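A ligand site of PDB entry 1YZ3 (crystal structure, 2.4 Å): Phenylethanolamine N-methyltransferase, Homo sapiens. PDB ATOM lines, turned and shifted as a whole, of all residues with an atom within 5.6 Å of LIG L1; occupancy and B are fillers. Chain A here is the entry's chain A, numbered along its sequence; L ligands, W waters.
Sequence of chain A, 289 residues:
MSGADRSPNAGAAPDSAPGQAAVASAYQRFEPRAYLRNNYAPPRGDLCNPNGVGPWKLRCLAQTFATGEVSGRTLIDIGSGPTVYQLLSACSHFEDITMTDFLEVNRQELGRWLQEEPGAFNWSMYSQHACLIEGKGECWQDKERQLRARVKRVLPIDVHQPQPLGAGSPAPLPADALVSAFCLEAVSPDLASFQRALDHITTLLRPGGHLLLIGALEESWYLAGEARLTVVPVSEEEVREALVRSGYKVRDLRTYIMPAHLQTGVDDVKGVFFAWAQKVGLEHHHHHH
The side-chain carboxylate (OD2) of Asp 101 sits at hydrogen-bond distance from the backbone NH (N) of Leu 103, at 3.3 Å.
The backbone carbonyl oxygen (O) of Ser 80 sits at hydrogen-bond distance from the side-chain hydroxyl (OG1) of Thr 83 (3.3 Å).
O of Ser 80 is in hydrogen-bond range of NE2 of Gln 86, 3.5 Å away.
The backbone carbonyl oxygen of Val 187 sits close to a ring nitrogen (NE2) of His 160, 3.5 Å away.
OD1 of Asp 158 sits at hydrogen-bond distance from N of His 160, 2.7 Å away.
OH of Tyr 27 is in hydrogen-bond range of OH of Tyr 222 (2.7 Å).
The side-chain hydroxyl (OH) of Tyr 27 sits at hydrogen-bond distance from the backbone carbonyl oxygen (O) of Ala 186.
The side-chain amide nitrogen of Gln 86 is in hydrogen-bond range of the side-chain carboxylate of Asp 77 (3.1 Å).
The backbone carbonyl oxygen of Phe 182 sits close to a sulfur (S1) of LIG L1 (3.5 Å).
Residues that only touch LIG L1: Tyr 27 (3.8 Å), Ser 80 (3.3 Å), Gly 81 (3.0 Å), Thr 83 (3.4 Å), Gln 86 (3.9 Å), Phe 102 (3.5 Å), Leu 103 (3.6 Å), Ile 157 (3.9 Å), Val 187 (3.4 Å) and Tyr 222 (3.9 Å).
Within 4 Å of LIG L1: Tyr 27, Tyr 35, Tyr 40, Gly 79, Ser 80, Gly 81, Thr 83, Tyr 85, Gln 86, Asp 101, Phe 102, Leu 103, Asn 106, Ile 157, Asp 158, Val 159, Ala 181, Phe 182, Cys 183, Val 187 and Tyr 222.
The nearest printed residue that does not touch LIG L1 is His 160 (4.03 Å).
The backbone carbonyl oxygen of Ala 181 lies within hydrogen-bond range of a nitrogen (N1) of LIG L1.
The side-chain hydroxyl of Tyr 35 is in hydrogen-bond range of an oxygen (O2) of LIG L1 (2.6 Å).
OH of Tyr 40 is in hydrogen-bond range of O2 of LIG L1, at 2.7 Å.
A nitrogen (N1) of LIG L1 is in hydrogen-bond range of the backbone carbonyl oxygen of Gly 79.
The side-chain carboxylate (OD1) of Asp 101 lies within hydrogen-bond range of an oxygen (O4) of LIG L1, 2.9 Å away.
The side-chain hydroxyl (OH) of Tyr 85 sits at hydrogen-bond distance from an oxygen (O1) of LIG L1 (2.9 Å).
An oxygen (O4) of LIG L1 sits at hydrogen-bond distance from the side-chain amide oxygen (OD1) of Asn 106, 2.9 Å away.
N of Val 159 is in hydrogen-bond range of N5 of LIG L1.
N6 of LIG L1 is in hydrogen-bond range of SG of Cys 183, at 3.4 Å.
N4 of LIG L1 is in hydrogen-bond range of OD1 of Asp 158, 3.5 Å away.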
ATOM      1  N   TYR A  27      27.588  16.067   9.478  1.00  0.00           N
ATOM      2  CA  TYR A  27      27.289  14.657   9.735  1.00  0.00           C
ATOM      3  C   TYR A  27      26.952  14.340  11.185  1.00  0.00           C
ATOM      4  O   TYR A  27      26.628  13.201  11.520  1.00  0.00           O
ATOM      5  CB  TYR A  27      28.435  13.761   9.278  1.00  0.00           C
ATOM      6  CG  TYR A  27      28.363  13.429   7.805  1.00  0.00           C
ATOM      7  CD1 TYR A  27      29.176  14.074   6.881  1.00  0.00           C
ATOM      8  CD2 TYR A  27      27.416  12.521   7.334  1.00  0.00           C
ATOM      9  CE1 TYR A  27      29.047  13.841   5.517  1.00  0.00           C
ATOM     10  CE2 TYR A  27      27.274  12.273   5.968  1.00  0.00           C
ATOM     11  CZ  TYR A  27      28.093  12.936   5.067  1.00  0.00           C
ATOM     12  OH  TYR A  27      27.953  12.723   3.725  1.00  0.00           O
ATOM     13  N   PHE A  30      23.381  13.708  11.088  1.00  0.00           N
ATOM     14  CA  PHE A  30      23.017  12.600  10.194  1.00  0.00           C
ATOM     15  C   PHE A  30      22.212  11.562  10.966  1.00  0.00           C
ATOM     16  O   PHE A  30      22.724  10.943  11.891  1.00  0.00           O
ATOM     17  CB  PHE A  30      24.288  11.952   9.640  1.00  0.00           C
ATOM     18  CG  PHE A  30      24.034  10.843   8.640  1.00  0.00           C
ATOM     19  CD1 PHE A  30      24.082  11.089   7.274  1.00  0.00           C
ATOM     20  CD2 PHE A  30      23.762   9.545   9.083  1.00  0.00           C
ATOM     21  CE1 PHE A  30      23.866  10.070   6.353  1.00  0.00           C
ATOM     22  CE2 PHE A  30      23.551   8.522   8.169  1.00  0.00           C
ATOM     23  CZ  PHE A  30      23.605   8.776   6.804  1.00  0.00           C
ATOM     24  N   TYR A  35      17.948   8.341   6.734  1.00  0.00           N
ATOM     25  CA  TYR A  35      18.782   8.032   5.583  1.00  0.00           C
ATOM     26  C   TYR A  35      18.301   6.732   4.933  1.00  0.00           C
ATOM     27  O   TYR A  35      18.193   6.648   3.714  1.00  0.00           O
ATOM     28  CB  TYR A  35      20.233   7.863   6.020  1.00  0.00           C
ATOM     29  CG  TYR A  35      21.149   7.497   4.871  1.00  0.00           C
ATOM     30  CD1 TYR A  35      21.619   8.472   3.996  1.00  0.00           C
ATOM     31  CD2 TYR A  35      21.534   6.174   4.666  1.00  0.00           C
ATOM     32  CE1 TYR A  35      22.462   8.131   2.928  1.00  0.00           C
ATOM     33  CE2 TYR A  35      22.371   5.825   3.598  1.00  0.00           C
ATOM     34  CZ  TYR A  35      22.822   6.800   2.749  1.00  0.00           C
ATOM     35  OH  TYR A  35      23.658   6.462   1.703  1.00  0.00           O
ATOM     36  N   TYR A  40      16.462   3.614   0.954  1.00  0.00           N
ATOM     37  CA  TYR A  40      16.264   2.176   0.839  1.00  0.00           C
ATOM     38  C   TYR A  40      14.871   1.698   1.189  1.00  0.00           C
ATOM     39  O   TYR A  40      14.681   0.541   1.518  1.00  0.00           O
ATOM     40  CB  TYR A  40      17.331   1.460   1.659  1.00  0.00           C
ATOM     41  CG  TYR A  40      18.707   1.862   1.183  1.00  0.00           C
ATOM     42  CD1 TYR A  40      19.341   3.000   1.683  1.00  0.00           C
ATOM     43  CD2 TYR A  40      19.328   1.153   0.157  1.00  0.00           C
ATOM     44  CE1 TYR A  40      20.570   3.423   1.170  1.00  0.00           C
ATOM     45  CE2 TYR A  40      20.551   1.568  -0.357  1.00  0.00           C
ATOM     46  CZ  TYR A  40      21.167   2.708   0.143  1.00  0.00           C
ATOM     47  OH  TYR A  40      22.361   3.110  -0.388  1.00  0.00           O
ATOM     48  N   LYS A  57      22.083  -1.423  -8.975  1.00  0.00           N
ATOM     49  CA  LYS A  57      23.272  -1.525  -8.138  1.00  0.00           C
ATOM     50  C   LYS A  57      23.635  -2.978  -7.842  1.00  0.00           C
ATOM     51  O   LYS A  57      24.801  -3.368  -7.961  1.00  0.00           O
ATOM     52  CB  LYS A  57      23.069  -0.751  -6.826  1.00  0.00           C
ATOM     53  CG  LYS A  57      23.258   0.761  -6.948  1.00  0.00           C
ATOM     54  CD  LYS A  57      23.288   1.452  -5.577  1.00  0.00           C
ATOM     55  CE  LYS A  57      21.963   1.305  -4.847  1.00  0.00           C
ATOM     56  NZ  LYS A  57      21.900   2.114  -3.609  1.00  0.00           N
ATOM     57  N   ASP A  77      35.008  -2.440   3.661  1.00  0.00           N
ATOM     58  CA  ASP A  77      33.939  -1.611   3.118  1.00  0.00           C
ATOM     59  C   ASP A  77      34.072  -0.211   3.687  1.00  0.00           C
ATOM     60  O   ASP A  77      33.793   0.015   4.869  1.00  0.00           O
ATOM     61  CB  ASP A  77      32.571  -2.215   3.476  1.00  0.00           C
ATOM     62  CG  ASP A  77      31.421  -1.452   2.845  1.00  0.00           C
ATOM     63  OD1 ASP A  77      31.559  -1.004   1.682  1.00  0.00           O
ATOM     64  OD2 ASP A  77      30.371  -1.312   3.511  1.00  0.00           O
ATOM     65  N   ILE A  78      34.508   0.723   2.850  1.00  0.00           N
ATOM     66  CA  ILE A  78      34.721   2.118   3.233  1.00  0.00           C
ATOM     67  C   ILE A  78      33.420   2.921   3.340  1.00  0.00           C
ATOM     68  O   ILE A  78      32.675   3.048   2.378  1.00  0.00           O
ATOM     69  CB  ILE A  78      35.639   2.832   2.199  1.00  0.00           C
ATOM     70  CG1 ILE A  78      36.877   1.983   1.922  1.00  0.00           C
ATOM     71  CG2 ILE A  78      36.032   4.192   2.727  1.00  0.00           C
ATOM     72  CD1 ILE A  78      37.748   1.725   3.126  1.00  0.00           C
ATOM     73  N   GLY A  79      33.162   3.494   4.523  1.00  0.00           N
ATOM     74  CA  GLY A  79      31.972   4.299   4.723  1.00  0.00           C
ATOM     75  C   GLY A  79      30.672   3.536   4.501  1.00  0.00           C
ATOM     76  O   GLY A  79      29.830   3.947   3.691  1.00  0.00           O
ATOM     77  N   SER A  80      30.521   2.433   5.219  1.00  0.00           N
ATOM     78  CA  SER A  80      29.363   1.565   5.120  1.00  0.00           C
ATOM     79  C   SER A  80      28.062   2.241   5.532  1.00  0.00           C
ATOM     80  O   SER A  80      26.978   1.845   5.105  1.00  0.00           O
ATOM     81  CB  SER A  80      29.568   0.331   6.002  1.00  0.00           C
ATOM     82  OG  SER A  80      30.861  -0.207   5.803  1.00  0.00           O
ATOM     83  N   GLY A  81      28.172   3.252   6.382  1.00  0.00           N
ATOM     84  CA  GLY A  81      26.971   3.917   6.857  1.00  0.00           C
ATOM     85  C   GLY A  81      26.151   2.849   7.548  1.00  0.00           C
ATOM     86  O   GLY A  81      26.711   1.961   8.183  1.00  0.00           O
ATOM     87  N   PRO A  82      24.814   2.895   7.465  1.00  0.00           N
ATOM     88  CA  PRO A  82      23.999   1.878   8.132  1.00  0.00           C
ATOM     89  C   PRO A  82      23.471   0.826   7.139  1.00  0.00           C
ATOM     90  O   PRO A  82      22.470   0.175   7.418  1.00  0.00           O
ATOM     91  CB  PRO A  82      22.878   2.696   8.742  1.00  0.00           C
ATOM     92  CG  PRO A  82      22.597   3.669   7.619  1.00  0.00           C
ATOM     93  CD  PRO A  82      23.980   4.079   7.129  1.00  0.00           C
ATOM     94  N   THR A  83      24.147   0.670   6.009  1.00  0.00           N
ATOM     95  CA  THR A  83      23.687  -0.267   4.992  1.00  0.00           C
ATOM     96  C   THR A  83      24.587  -1.491   4.747  1.00  0.00           C
ATOM     97  O   THR A  83      25.806  -1.424   4.922  1.00  0.00           O
ATOM     98  CB  THR A  83      23.477   0.477   3.647  1.00  0.00           C
ATOM     99  OG1 THR A  83      24.730   0.626   2.969  1.00  0.00           O
ATOM    100  CG2 THR A  83      22.886   1.874   3.907  1.00  0.00           C
ATOM    101  N   TYR A  85      23.565  -3.869   1.945  1.00  0.00           N
ATOM    102  CA  TYR A  85      23.290  -4.333   0.593  1.00  0.00           C
ATOM    103  C   TYR A  85      24.537  -4.416  -0.297  1.00  0.00           C
ATOM    104  O   TYR A  85      24.659  -5.335  -1.120  1.00  0.00           O
ATOM    105  CB  TYR A  85      22.271  -3.401  -0.082  1.00  0.00           C
ATOM    106  CG  TYR A  85      22.883  -2.117  -0.589  1.00  0.00           C
ATOM    107  CD1 TYR A  85      23.439  -2.053  -1.863  1.00  0.00           C
ATOM    108  CD2 TYR A  85      22.947  -0.984   0.208  1.00  0.00           C
ATOM    109  CE1 TYR A  85      24.042  -0.911  -2.322  1.00  0.00           C
ATOM    110  CE2 TYR A  85      23.551   0.170  -0.243  1.00  0.00           C
ATOM    111  CZ  TYR A  85      24.098   0.200  -1.505  1.00  0.00           C
ATOM    112  OH  TYR A  85      24.690   1.352  -1.965  1.00  0.00           O
ATOM    113  N   GLN A  86      25.453  -3.473  -0.131  1.00  0.00           N
ATOM    114  CA  GLN A  86      26.665  -3.420  -0.931  1.00  0.00           C
ATOM    115  C   GLN A  86      27.615  -4.609  -0.708  1.00  0.00           C
ATOM    116  O   GLN A  86      28.636  -4.750  -1.383  1.00  0.00           O
ATOM    117  CB  GLN A  86      27.408  -2.097  -0.674  1.00  0.00           C
ATOM    118  CG  GLN A  86      27.982  -1.924   0.729  1.00  0.00           C
ATOM    119  CD  GLN A  86      26.998  -1.301   1.712  1.00  0.00           C
ATOM    120  OE1 GLN A  86      25.783  -1.495   1.601  1.00  0.00           O
ATOM    121  NE2 GLN A  86      27.520  -0.567   2.685  1.00  0.00           N
ATOM    122  N   ASP A 101      32.918   3.065   9.245  1.00  0.00           N
ATOM    123  CA  ASP A 101      32.167   4.308   9.159  1.00  0.00           C
ATOM    124  C   ASP A 101      32.562   5.333  10.212  1.00  0.00           C
ATOM    125  O   ASP A 101      32.916   5.003  11.336  1.00  0.00           O
ATOM    126  CB  ASP A 101      30.667   4.082   9.226  1.00  0.00           C
ATOM    127  CG  ASP A 101      29.905   5.260   8.639  1.00  0.00           C
ATOM    128  OD1 ASP A 101      30.026   5.496   7.412  1.00  0.00           O
ATOM    129  OD2 ASP A 101      29.207   5.959   9.404  1.00  0.00           O
ATOM    130  N   PHE A 102      32.464   6.595   9.793  1.00  0.00           N
ATOM    131  CA  PHE A 102      32.791   7.756  10.609  1.00  0.00           C
ATOM    132  C   PHE A 102      31.950   7.903  11.864  1.00  0.00           C
ATOM    133  O   PHE A 102      32.497   8.082  12.953  1.00  0.00           O
ATOM    134  CB  PHE A 102      32.625   9.006   9.753  1.00  0.00           C
ATOM    135  CG  PHE A 102      33.114  10.260  10.407  1.00  0.00           C
ATOM    136  CD1 PHE A 102      34.486  10.489  10.559  1.00  0.00           C
ATOM    137  CD2 PHE A 102      32.222  11.219  10.856  1.00  0.00           C
ATOM    138  CE1 PHE A 102      34.953  11.662  11.157  1.00  0.00           C
ATOM    139  CE2 PHE A 102      32.679  12.401  11.454  1.00  0.00           C
ATOM    140  CZ  PHE A 102      34.038  12.615  11.604  1.00  0.00           C
ATOM    141  N   LEU A 103      30.626   7.843  11.711  1.00  0.00           N
ATOM    142  CA  LEU A 103      29.720   8.020  12.849  1.00  0.00           C
ATOM    143  C   LEU A 103      29.480   6.791  13.710  1.00  0.00           C
ATOM    144  O   LEU A 103      29.331   5.683  13.200  1.00  0.00           O
ATOM    145  CB  LEU A 103      28.369   8.554  12.355  1.00  0.00           C
ATOM    146  CG  LEU A 103      28.366   9.902  11.636  1.00  0.00           C
ATOM    147  CD1 LEU A 103      26.951  10.226  11.167  1.00  0.00           C
ATOM    148  CD2 LEU A 103      28.888  10.992  12.573  1.00  0.00           C
ATOM    149  N   ASN A 106      25.929   5.221  13.131  1.00  0.00           N
ATOM    150  CA  ASN A 106      25.836   4.292  12.017  1.00  0.00           C
ATOM    151  C   ASN A 106      26.355   2.919  12.414  1.00  0.00           C
ATOM    152  O   ASN A 106      25.709   1.912  12.112  1.00  0.00           O
ATOM    153  CB  ASN A 106      26.625   4.805  10.822  1.00  0.00           C
ATOM    154  CG  ASN A 106      25.866   5.860  10.050  1.00  0.00           C
ATOM    155  OD1 ASN A 106      26.452   6.622   9.282  1.00  0.00           O
ATOM    156  ND2 ASN A 106      24.552   5.895  10.237  1.00  0.00           N
ATOM    157  N   ILE A 157      36.409   5.189  10.883  1.00  0.00           N
ATOM    158  CA  ILE A 157      37.279   5.523   9.760  1.00  0.00           C
ATOM    159  C   ILE A 157      37.116   6.994   9.349  1.00  0.00           C
ATOM    160  O   ILE A 157      36.092   7.613   9.627  1.00  0.00           O
ATOM    161  CB  ILE A 157      36.956   4.614   8.540  1.00  0.00           C
ATOM    162  CG1 ILE A 157      37.993   4.807   7.440  1.00  0.00           C
ATOM    163  CG2 ILE A 157      35.560   4.916   8.015  1.00  0.00           C
ATOM    164  CD1 ILE A 157      37.827   3.866   6.272  1.00  0.00           C
ATOM    165  N   ASP A 158      38.153   7.537   8.718  1.00  0.00           N
ATOM    166  CA  ASP A 158      38.161   8.913   8.249  1.00  0.00           C
ATOM    167  C   ASP A 158      39.006   8.905   6.989  1.00  0.00           C
ATOM    168  O   ASP A 158      40.223   9.012   7.053  1.00  0.00           O
ATOM    169  CB  ASP A 158      38.793   9.849   9.284  1.00  0.00           C
ATOM    170  CG  ASP A 158      38.681  11.314   8.891  1.00  0.00           C
ATOM    171  OD1 ASP A 158      38.892  11.640   7.703  1.00  0.00           O
ATOM    172  OD2 ASP A 158      38.391  12.143   9.782  1.00  0.00           O
ATOM    173  N   VAL A 159      38.357   8.779   5.840  1.00  0.00           N
ATOM    174  CA  VAL A 159      39.060   8.721   4.561  1.00  0.00           C
ATOM    175  C   VAL A 159      39.909   9.963   4.308  1.00  0.00           C
ATOM    176  O   VAL A 159      40.630  10.053   3.316  1.00  0.00           O
ATOM    177  CB  VAL A 159      38.059   8.546   3.414  1.00  0.00           C
ATOM    178  CG1 VAL A 159      37.378   7.193   3.543  1.00  0.00           C
ATOM    179  CG2 VAL A 159      37.012   9.655   3.457  1.00  0.00           C
ATOM    180  N   HIS A 160      39.824  10.918   5.227  1.00  0.00           N
ATOM    181  CA  HIS A 160      40.590  12.139   5.074  1.00  0.00           C
ATOM    182  C   HIS A 160      41.945  12.034   5.765  1.00  0.00           C
ATOM    183  O   HIS A 160      42.923  12.643   5.318  1.00  0.00           O
ATOM    184  CB  HIS A 160      39.750  13.306   5.603  1.00  0.00           C
ATOM    185  CG  HIS A 160      38.708  13.784   4.628  1.00  0.00           C
ATOM    186  ND1 HIS A 160      37.571  14.446   5.014  1.00  0.00           N
ATOM    187  CD2 HIS A 160      38.673  13.720   3.273  1.00  0.00           C
ATOM    188  CE1 HIS A 160      36.865  14.774   3.939  1.00  0.00           C
ATOM    189  NE2 HIS A 160      37.515  14.333   2.867  1.00  0.00           N
ATOM    190  N   ALA A 181      30.482   2.624  -1.310  1.00  0.00           N
ATOM    191  CA  ALA A 181      29.332   3.186  -2.009  1.00  0.00           C
ATOM    192  C   ALA A 181      28.859   4.467  -1.365  1.00  0.00           C
ATOM    193  O   ALA A 181      28.623   4.511  -0.157  1.00  0.00           O
ATOM    194  CB  ALA A 181      28.176   2.178  -2.039  1.00  0.00           C
ATOM    195  N   PHE A 182      28.728   5.504  -2.197  1.00  0.00           N
ATOM    196  CA  PHE A 182      28.260   6.819  -1.771  1.00  0.00           C
ATOM    197  C   PHE A 182      28.996   7.416  -0.580  1.00  0.00           C
ATOM    198  O   PHE A 182      28.389   8.039   0.293  1.00  0.00           O
ATOM    199  CB  PHE A 182      26.754   6.779  -1.472  1.00  0.00           C
ATOM    200  CG  PHE A 182      25.926   6.238  -2.602  1.00  0.00           C
ATOM    201  CD1 PHE A 182      25.499   4.912  -2.604  1.00  0.00           C
ATOM    202  CD2 PHE A 182      25.573   7.057  -3.682  1.00  0.00           C
ATOM    203  CE1 PHE A 182      24.726   4.406  -3.650  1.00  0.00           C
ATOM    204  CE2 PHE A 182      24.802   6.564  -4.734  1.00  0.00           C
ATOM    205  CZ  PHE A 182      24.373   5.237  -4.722  1.00  0.00           C
ATOM    206  N   CYS A 183      30.316   7.247  -0.555  1.00  0.00           N
ATOM    207  CA  CYS A 183      31.088   7.798   0.550  1.00  0.00           C
ATOM    208  C   CYS A 183      31.969   8.978   0.147  1.00  0.00           C
ATOM    209  O   CYS A 183      31.730  10.104   0.576  1.00  0.00           O
ATOM    210  CB  CYS A 183      31.959   6.720   1.172  1.00  0.00           C
ATOM    211  SG  CYS A 183      32.827   7.305   2.655  1.00  0.00           S
ATOM    212  N   ALA A 186      30.454  12.106  -1.115  1.00  0.00           N
ATOM    213  CA  ALA A 186      29.555  12.644  -0.110  1.00  0.00           C
ATOM    214  C   ALA A 186      30.217  13.231   1.139  1.00  0.00           C
ATOM    215  O   ALA A 186      29.554  13.840   1.972  1.00  0.00           O
ATOM    216  CB  ALA A 186      28.548  11.568   0.299  1.00  0.00           C
ATOM    217  N   VAL A 187      31.535  13.051   1.270  1.00  0.00           N
ATOM    218  CA  VAL A 187      32.236  13.561   2.453  1.00  0.00           C
ATOM    219  C   VAL A 187      33.387  14.513   2.095  1.00  0.00           C
ATOM    220  O   VAL A 187      34.119  14.979   2.973  1.00  0.00           O
ATOM    221  CB  VAL A 187      32.798  12.402   3.291  1.00  0.00           C
ATOM    222  CG1 VAL A 187      31.694  11.417   3.593  1.00  0.00           C
ATOM    223  CG2 VAL A 187      33.942  11.709   2.556  1.00  0.00           C
ATOM    224  N   TYR A 222      22.038  16.327  -0.189  1.00  0.00           N
ATOM    225  CA  TYR A 222      21.099  15.243   0.139  1.00  0.00           C
ATOM    226  C   TYR A 222      20.785  15.332   1.629  1.00  0.00           C
ATOM    227  O   TYR A 222      21.624  15.758   2.433  1.00  0.00           O
ATOM    228  CB  TYR A 222      21.681  13.866  -0.228  1.00  0.00           C
ATOM    229  CG  TYR A 222      22.743  13.323   0.716  1.00  0.00           C
ATOM    230  CD1 TYR A 222      22.380  12.594   1.855  1.00  0.00           C
ATOM    231  CD2 TYR A 222      24.099  13.471   0.442  1.00  0.00           C
ATOM    232  CE1 TYR A 222      23.342  12.016   2.690  1.00  0.00           C
ATOM    233  CE2 TYR A 222      25.079  12.904   1.273  1.00  0.00           C
ATOM    234  CZ  TYR A 222      24.683  12.179   2.396  1.00  0.00           C
ATOM    235  OH  TYR A 222      25.615  11.576   3.206  1.00  0.00           O
HETATM  236  N1  LIG L   1      27.661   3.306   1.958  1.00  0.00           N
HETATM  237  C1  LIG L   1      26.310   3.600   2.436  1.00  0.00           C
HETATM  238  C2  LIG L   1      26.277   4.980   3.136  1.00  0.00           C
HETATM  239  C3  LIG L   1      26.734   6.195   2.310  1.00  0.00           C
HETATM  240  S1  LIG L   1      26.395   7.795   3.181  1.00  0.00           S
HETATM  241  C4  LIG L   1      25.286   3.510   1.293  1.00  0.00           C
HETATM  242  O1  LIG L   1      25.667   3.032   0.202  1.00  0.00           O
HETATM  243  O2  LIG L   1      24.107   3.874   1.503  1.00  0.00           O
HETATM  244  C5  LIG L   1      28.095   8.444   3.436  1.00  0.00           C
HETATM  245  C6  LIG L   1      28.712   7.857   4.689  1.00  0.00           C
HETATM  246  O3  LIG L   1      30.080   8.304   4.897  1.00  0.00           O
HETATM  247  C7  LIG L   1      27.964   8.117   5.999  1.00  0.00           C
HETATM  248  O4  LIG L   1      27.645   6.877   6.627  1.00  0.00           O
HETATM  249  C8  LIG L   1      28.925   8.991   6.789  1.00  0.00           C
HETATM  250  O5  LIG L   1      28.831   8.856   8.194  1.00  0.00           O
HETATM  251  C9  LIG L   1      30.288   8.522   6.279  1.00  0.00           C
HETATM  252  N2  LIG L   1      31.382   9.470   6.478  1.00  0.00           N
HETATM  253  C10 LIG L   1      31.312  10.833   6.912  1.00  0.00           C
HETATM  254  N3  LIG L   1      32.487  11.411   7.023  1.00  0.00           N
HETATM  255  C11 LIG L   1      33.371  10.399   6.641  1.00  0.00           C
HETATM  256  C12 LIG L   1      34.794  10.442   6.572  1.00  0.00           C
HETATM  257  N4  LIG L   1      35.532  11.504   6.876  1.00  0.00           N
HETATM  258  N5  LIG L   1      35.420   9.307   6.159  1.00  0.00           N
HETATM  259  C13 LIG L   1      34.670   8.218   5.846  1.00  0.00           C
HETATM  260  N6  LIG L   1      33.322   8.077   5.893  1.00  0.00           N
HETATM  261  C14 LIG L   1      32.731   9.222   6.301  1.00  0.00           C
HETATM  262 CL1  LG2 L   2      20.886   8.074  -5.574  1.00  0.00          CL
HETATM  263  C1  LG2 L   2      21.337   7.470  -4.006  1.00  0.00           C
HETATM  264  C2  LG2 L   2      21.946   8.320  -3.084  1.00  0.00           C
HETATM  265  C3  LG2 L   2      22.254   9.784  -3.422  1.00  0.00           C
HETATM  266  N1  LG2 L   2      22.486  10.572  -2.195  1.00  0.00           N
HETATM  267  C4  LG2 L   2      23.533   9.964  -1.370  1.00  0.00           C
HETATM  268  C5  LG2 L   2      22.978   8.661  -0.761  1.00  0.00           C
HETATM  269  C6  LG2 L   2      22.314   7.809  -1.843  1.00  0.00           C
HETATM  270  C7  LG2 L   2      22.070   6.477  -1.528  1.00  0.00           C
HETATM  271  C8  LG2 L   2      21.456   5.632  -2.457  1.00  0.00           C
HETATM  272  C9  LG2 L   2      21.087   6.130  -3.692  1.00  0.00           C
HETATM  273 CL2  LG2 L   2      20.333   5.058  -4.821  1.00  0.00          CL
HETATM  274  O   HOH W   1      30.164   1.563   1.395  1.00  0.00           O
HETATM  275  O   HOH W   2      34.372  13.960   8.130  1.00  0.00           O
